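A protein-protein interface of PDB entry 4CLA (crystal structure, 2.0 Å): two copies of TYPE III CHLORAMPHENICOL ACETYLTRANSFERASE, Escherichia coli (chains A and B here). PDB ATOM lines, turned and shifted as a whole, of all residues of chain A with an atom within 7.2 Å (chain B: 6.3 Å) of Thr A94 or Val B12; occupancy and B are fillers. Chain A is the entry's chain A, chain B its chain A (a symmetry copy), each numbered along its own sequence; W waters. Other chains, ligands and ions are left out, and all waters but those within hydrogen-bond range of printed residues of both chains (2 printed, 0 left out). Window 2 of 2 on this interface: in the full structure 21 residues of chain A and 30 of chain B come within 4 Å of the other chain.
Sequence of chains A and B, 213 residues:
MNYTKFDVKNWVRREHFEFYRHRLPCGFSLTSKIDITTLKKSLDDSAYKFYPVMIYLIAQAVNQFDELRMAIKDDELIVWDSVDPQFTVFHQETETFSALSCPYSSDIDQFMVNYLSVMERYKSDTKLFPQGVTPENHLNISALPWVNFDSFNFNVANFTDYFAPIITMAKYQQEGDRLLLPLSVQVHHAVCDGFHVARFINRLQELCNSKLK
Of the printed residues of chain B, Thr A94 touches Val B12 (3.6 Å). Printed residues of chain B within 4 Å of Thr A96: Val B12 and Arg B13. Printed residues of chain B within 4 Å of Phe A97: His B16 (2.9 Å). Trp B11 touches none of the printed residues of chain A. Printed residues of chain A within 4 Å of Val B12: Thr A94 and Thr A96. Of the printed residues of chain A, Arg B13 touches Thr A96 (3.7 Å). Printed residues of chain A within 4 Å of His B16: Phe A97 (2.9 Å).
The backbone carbonyl oxygen (O) of Phe A97 lies within hydrogen-bond range of a ring nitrogen (NE2) of His B16 (2.9 Å).
N of His A91 sits at hydrogen-bond distance from O of Thr A96, at 2.8 Å. The side-chain hydroxyl (OG1) of Thr A94 lies within hydrogen-bond range of the side-chain hydroxyl (OG1) of Thr A96 (2.7 Å).
No position is printed for both chains. Of the 4 pairs that touch across the chains among the printed residues, none has its exchanged pair printed and touching as well.
Water W2 lies within hydrogen-bond range of OE1 of Glu B15 (2.6 Å) and O of Thr A126 (2.9 Å). Water W1 bridges N of Phe A97 (3.1 Å) and NE2 of His B16 (3.2 Å).
Of the 8 printed residues of chain B, 3 touch a printed residue of chain A. Of the 9 printed residues of chain A, 3 touch a printed residue of chain B. Along chain A the printed residues that touch a printed residue of chain B span positions 94 to 97. Among the printed residues, 4 pairs touch across the chains. Among the printed residues, no Asp or Glu carboxylate lies within 4 Å of a Lys or Arg side-chain nitrogen of the other chain.
Among the printed residues, pairs that only touch across the chains: Thr A94 with Val B12 (3.6 Å), Thr A96 with Val B12 (3.6 Å) and Thr A96 with Arg B13 (3.7 Å).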
ATOM      1  N   PHE A  90      -4.074 -16.878 -11.315  1.00  0.00           N
ATOM      2  CA  PHE A  90      -4.420 -17.139  -9.927  1.00  0.00           C
ATOM      3  C   PHE A  90      -5.855 -17.688  -9.861  1.00  0.00           C
ATOM      4  O   PHE A  90      -6.695 -17.106 -10.488  1.00  0.00           O
ATOM      5  CB  PHE A  90      -4.402 -15.858  -9.108  1.00  0.00           C
ATOM      6  CG  PHE A  90      -4.564 -15.941  -7.637  1.00  0.00           C
ATOM      7  CD1 PHE A  90      -3.651 -16.677  -6.860  1.00  0.00           C
ATOM      8  CD2 PHE A  90      -5.706 -15.421  -7.021  1.00  0.00           C
ATOM      9  CE1 PHE A  90      -3.835 -16.750  -5.466  1.00  0.00           C
ATOM     10  CE2 PHE A  90      -5.855 -15.490  -5.607  1.00  0.00           C
ATOM     11  CZ  PHE A  90      -4.900 -16.113  -4.812  1.00  0.00           C
ATOM     12  N   HIS A  91      -6.053 -18.686  -9.006  1.00  0.00           N
ATOM     13  CA  HIS A  91      -7.397 -19.264  -8.847  1.00  0.00           C
ATOM     14  C   HIS A  91      -7.874 -18.755  -7.489  1.00  0.00           C
ATOM     15  O   HIS A  91      -7.355 -19.188  -6.457  1.00  0.00           O
ATOM     16  CB  HIS A  91      -7.353 -20.805  -8.807  1.00  0.00           C
ATOM     17  CG  HIS A  91      -6.803 -21.336 -10.136  1.00  0.00           C
ATOM     18  ND1 HIS A  91      -7.415 -21.250 -11.339  1.00  0.00           N
ATOM     19  CD2 HIS A  91      -5.641 -22.015 -10.358  1.00  0.00           C
ATOM     20  CE1 HIS A  91      -6.677 -21.849 -12.272  1.00  0.00           C
ATOM     21  NE2 HIS A  91      -5.596 -22.328 -11.678  1.00  0.00           N
ATOM     22  N   GLN A  92      -8.894 -17.927  -7.506  1.00  0.00           N
ATOM     23  CA  GLN A  92      -9.371 -17.392  -6.211  1.00  0.00           C
ATOM     24  C   GLN A  92      -9.886 -18.442  -5.256  1.00  0.00           C
ATOM     25  O   GLN A  92      -9.820 -18.384  -4.006  1.00  0.00           O
ATOM     26  CB  GLN A  92     -10.530 -16.372  -6.504  1.00  0.00           C
ATOM     27  CG  GLN A  92     -10.486 -15.381  -5.275  1.00  0.00           C
ATOM     28  N   GLU A  93     -10.516 -19.450  -5.831  1.00  0.00           N
ATOM     29  CA  GLU A  93     -11.137 -20.529  -5.115  1.00  0.00           C
ATOM     30  C   GLU A  93     -10.120 -21.338  -4.320  1.00  0.00           C
ATOM     31  O   GLU A  93     -10.549 -21.661  -3.192  1.00  0.00           O
ATOM     32  CB  GLU A  93     -11.953 -21.548  -5.892  1.00  0.00           C
ATOM     33  CG  GLU A  93     -12.820 -20.974  -7.045  1.00  0.00           C
ATOM     34  CD  GLU A  93     -11.947 -20.467  -8.199  1.00  0.00           C
ATOM     35  OE1 GLU A  93     -12.003 -19.306  -8.548  1.00  0.00           O
ATOM     36  OE2 GLU A  93     -11.132 -21.346  -8.569  1.00  0.00           O
ATOM     37  N   THR A  94      -8.986 -21.691  -4.886  1.00  0.00           N
ATOM     38  CA  THR A  94      -8.055 -22.518  -4.091  1.00  0.00           C
ATOM     39  C   THR A  94      -6.901 -21.695  -3.544  1.00  0.00           C
ATOM     40  O   THR A  94      -6.052 -22.235  -2.805  1.00  0.00           O
ATOM     41  CB  THR A  94      -7.484 -23.632  -5.056  1.00  0.00           C
ATOM     42  OG1 THR A  94      -7.055 -22.886  -6.240  1.00  0.00           O
ATOM     43  CG2 THR A  94      -8.537 -24.641  -5.495  1.00  0.00           C
ATOM     44  N   GLU A  95      -6.815 -20.454  -4.037  1.00  0.00           N
ATOM     45  CA  GLU A  95      -5.675 -19.560  -3.702  1.00  0.00           C
ATOM     46  C   GLU A  95      -4.341 -20.196  -4.150  1.00  0.00           C
ATOM     47  O   GLU A  95      -3.286 -20.191  -3.497  1.00  0.00           O
ATOM     48  CB  GLU A  95      -5.620 -19.232  -2.202  1.00  0.00           C
ATOM     49  CG  GLU A  95      -6.725 -18.362  -1.686  1.00  0.00           C
ATOM     50  CD  GLU A  95      -6.820 -18.078  -0.202  1.00  0.00           C
ATOM     51  OE1 GLU A  95      -6.099 -18.538   0.669  1.00  0.00           O
ATOM     52  OE2 GLU A  95      -7.717 -17.210  -0.076  1.00  0.00           O
ATOM     53  N   THR A  96      -4.340 -20.775  -5.356  1.00  0.00           N
ATOM     54  CA  THR A  96      -3.161 -21.376  -5.967  1.00  0.00           C
ATOM     55  C   THR A  96      -2.995 -20.835  -7.356  1.00  0.00           C
ATOM     56  O   THR A  96      -3.933 -20.159  -7.811  1.00  0.00           O
ATOM     57  CB  THR A  96      -3.274 -22.950  -5.984  1.00  0.00           C
ATOM     58  OG1 THR A  96      -4.417 -23.242  -6.809  1.00  0.00           O
ATOM     59  CG2 THR A  96      -3.444 -23.523  -4.574  1.00  0.00           C
ATOM     60  N   PHE A  97      -1.868 -21.081  -8.006  1.00  0.00           N
ATOM     61  CA  PHE A  97      -1.735 -20.535  -9.384  1.00  0.00           C
ATOM     62  C   PHE A  97      -1.462 -21.697 -10.317  1.00  0.00           C
ATOM     63  O   PHE A  97      -1.033 -22.782  -9.904  1.00  0.00           O
ATOM     64  CB  PHE A  97      -0.637 -19.477  -9.448  1.00  0.00           C
ATOM     65  CG  PHE A  97       0.774 -20.030  -9.314  1.00  0.00           C
ATOM     66  CD1 PHE A  97       1.539 -20.353 -10.453  1.00  0.00           C
ATOM     67  CD2 PHE A  97       1.316 -20.219  -8.072  1.00  0.00           C
ATOM     68  CE1 PHE A  97       2.843 -20.839 -10.344  1.00  0.00           C
ATOM     69  CE2 PHE A  97       2.630 -20.727  -7.922  1.00  0.00           C
ATOM     70  CZ  PHE A  97       3.393 -20.997  -9.066  1.00  0.00           C
ATOM     71  N   THR A 126      -6.797 -26.467 -11.974  1.00  0.00           N
ATOM     72  CA  THR A 126      -5.808 -26.186 -10.924  1.00  0.00           C
ATOM     73  C   THR A 126      -4.520 -26.936 -11.034  1.00  0.00           C
ATOM     74  O   THR A 126      -3.610 -26.786 -10.182  1.00  0.00           O
ATOM     75  CB  THR A 126      -6.533 -26.313  -9.494  1.00  0.00           C
ATOM     76  OG1 THR A 126      -6.946 -27.716  -9.453  1.00  0.00           O
ATOM     77  CG2 THR A 126      -7.665 -25.300  -9.387  1.00  0.00           C
ATOM     78  N   VAL B   8      -0.537 -33.503   3.354  1.00  0.00           N
ATOM     79  CA  VAL B   8       0.031 -33.200   2.026  1.00  0.00           C
ATOM     80  C   VAL B   8      -0.776 -33.837   0.905  1.00  0.00           C
ATOM     81  O   VAL B   8      -0.907 -33.203  -0.161  1.00  0.00           O
ATOM     82  CB  VAL B   8       1.543 -33.462   1.903  1.00  0.00           C
ATOM     83  CG1 VAL B   8       2.133 -32.976   0.526  1.00  0.00           C
ATOM     84  CG2 VAL B   8       2.355 -32.806   2.988  1.00  0.00           C
ATOM     85  N   ASN B  10      -3.940 -34.304   0.437  1.00  0.00           N
ATOM     86  CA  ASN B  10      -5.161 -33.558   0.060  1.00  0.00           C
ATOM     87  C   ASN B  10      -4.916 -32.068   0.024  1.00  0.00           C
ATOM     88  O   ASN B  10      -5.862 -31.264   0.273  1.00  0.00           O
ATOM     89  CB  ASN B  10      -6.255 -33.931   1.157  1.00  0.00           C
ATOM     90  CG  ASN B  10      -6.616 -35.445   0.849  1.00  0.00           C
ATOM     91  N   TRP B  11      -3.679 -31.670  -0.165  1.00  0.00           N
ATOM     92  CA  TRP B  11      -3.455 -30.157  -0.105  1.00  0.00           C
ATOM     93  C   TRP B  11      -3.646 -29.658  -1.532  1.00  0.00           C
ATOM     94  O   TRP B  11      -3.157 -30.367  -2.414  1.00  0.00           O
ATOM     95  CB  TRP B  11      -2.046 -29.927   0.383  1.00  0.00           C
ATOM     96  CG  TRP B  11      -1.548 -28.572   0.640  1.00  0.00           C
ATOM     97  CD1 TRP B  11      -2.218 -27.379   0.828  1.00  0.00           C
ATOM     98  CD2 TRP B  11      -0.154 -28.252   0.759  1.00  0.00           C
ATOM     99  NE1 TRP B  11      -1.339 -26.353   1.070  1.00  0.00           N
ATOM    100  CE2 TRP B  11      -0.065 -26.883   1.048  1.00  0.00           C
ATOM    101  CE3 TRP B  11       0.995 -29.055   0.652  1.00  0.00           C
ATOM    102  CZ2 TRP B  11       1.167 -26.221   1.241  1.00  0.00           C
ATOM    103  CZ3 TRP B  11       2.200 -28.442   0.890  1.00  0.00           C
ATOM    104  CH2 TRP B  11       2.276 -27.077   1.191  1.00  0.00           C
ATOM    105  N   VAL B  12      -4.290 -28.499  -1.678  1.00  0.00           N
ATOM    106  CA  VAL B  12      -4.421 -27.964  -3.048  1.00  0.00           C
ATOM    107  C   VAL B  12      -3.044 -27.620  -3.669  1.00  0.00           C
ATOM    108  O   VAL B  12      -2.994 -27.514  -4.907  1.00  0.00           O
ATOM    109  CB  VAL B  12      -5.361 -26.727  -3.011  1.00  0.00           C
ATOM    110  CG1 VAL B  12      -6.773 -27.170  -2.599  1.00  0.00           C
ATOM    111  CG2 VAL B  12      -4.958 -25.597  -2.072  1.00  0.00           C
ATOM    112  N   ARG B  13      -2.020 -27.336  -2.888  1.00  0.00           N
ATOM    113  CA  ARG B  13      -0.695 -26.995  -3.341  1.00  0.00           C
ATOM    114  C   ARG B  13       0.157 -28.262  -3.396  1.00  0.00           C
ATOM    115  O   ARG B  13       1.397 -28.126  -3.482  1.00  0.00           O
ATOM    116  CB  ARG B  13       0.054 -25.938  -2.455  1.00  0.00           C
ATOM    117  CG  ARG B  13      -0.525 -24.544  -2.622  1.00  0.00           C
ATOM    118  CD  ARG B  13       0.220 -23.437  -1.954  1.00  0.00           C
ATOM    119  NE  ARG B  13       1.482 -23.068  -2.612  1.00  0.00           N
ATOM    120  CZ  ARG B  13       2.682 -23.615  -2.373  1.00  0.00           C
ATOM    121  NH1 ARG B  13       2.894 -24.591  -1.463  1.00  0.00           N
ATOM    122  NH2 ARG B  13       3.741 -23.088  -3.034  1.00  0.00           N
ATOM    123  N   ARG B  14      -0.351 -29.489  -3.316  1.00  0.00           N
ATOM    124  CA  ARG B  14       0.652 -30.586  -3.268  1.00  0.00           C
ATOM    125  C   ARG B  14       1.561 -30.669  -4.483  1.00  0.00           C
ATOM    126  O   ARG B  14       2.757 -31.057  -4.400  1.00  0.00           O
ATOM    127  CB  ARG B  14       0.060 -31.960  -2.959  1.00  0.00           C
ATOM    128  CG  ARG B  14      -1.026 -32.394  -3.854  1.00  0.00           C
ATOM    129  CD  ARG B  14      -1.439 -33.812  -3.564  1.00  0.00           C
ATOM    130  NE  ARG B  14      -2.533 -34.275  -4.377  1.00  0.00           N
ATOM    131  CZ  ARG B  14      -3.767 -33.799  -4.563  1.00  0.00           C
ATOM    132  NH1 ARG B  14      -4.227 -32.715  -3.938  1.00  0.00           N
ATOM    133  NH2 ARG B  14      -4.575 -34.466  -5.436  1.00  0.00           N
ATOM    134  N   GLU B  15       1.101 -30.356  -5.682  1.00  0.00           N
ATOM    135  CA  GLU B  15       1.980 -30.461  -6.845  1.00  0.00           C
ATOM    136  C   GLU B  15       3.060 -29.382  -6.782  1.00  0.00           C
ATOM    137  O   GLU B  15       4.245 -29.591  -7.067  1.00  0.00           O
ATOM    138  CB  GLU B  15       1.140 -30.209  -8.091  1.00  0.00           C
ATOM    139  CG  GLU B  15       1.829 -30.465  -9.415  1.00  0.00           C
ATOM    140  CD  GLU B  15       0.979 -30.148 -10.631  1.00  0.00           C
ATOM    141  OE1 GLU B  15      -0.150 -29.657 -10.592  1.00  0.00           O
ATOM    142  OE2 GLU B  15       1.669 -30.375 -11.676  1.00  0.00           O
ATOM    143  N   HIS B  16       2.627 -28.184  -6.380  1.00  0.00           N
ATOM    144  CA  HIS B  16       3.578 -27.029  -6.267  1.00  0.00           C
ATOM    145  C   HIS B  16       4.692 -27.318  -5.226  1.00  0.00           C
ATOM    146  O   HIS B  16       5.868 -26.956  -5.440  1.00  0.00           O
ATOM    147  CB  HIS B  16       2.827 -25.781  -5.703  1.00  0.00           C
ATOM    148  CG  HIS B  16       1.684 -25.434  -6.633  1.00  0.00           C
ATOM    149  ND1 HIS B  16       0.509 -26.137  -6.633  1.00  0.00           N
ATOM    150  CD2 HIS B  16       1.558 -24.475  -7.566  1.00  0.00           C
ATOM    151  CE1 HIS B  16      -0.313 -25.607  -7.541  1.00  0.00           C
ATOM    152  NE2 HIS B  16       0.289 -24.578  -8.108  1.00  0.00           N
HETATM  153  O   HOH W   1      -0.110 -22.394  -5.870  1.00  0.00           O
HETATM  154  O   HOH W   2      -1.938 -28.755  -8.966  1.00  0.00           O
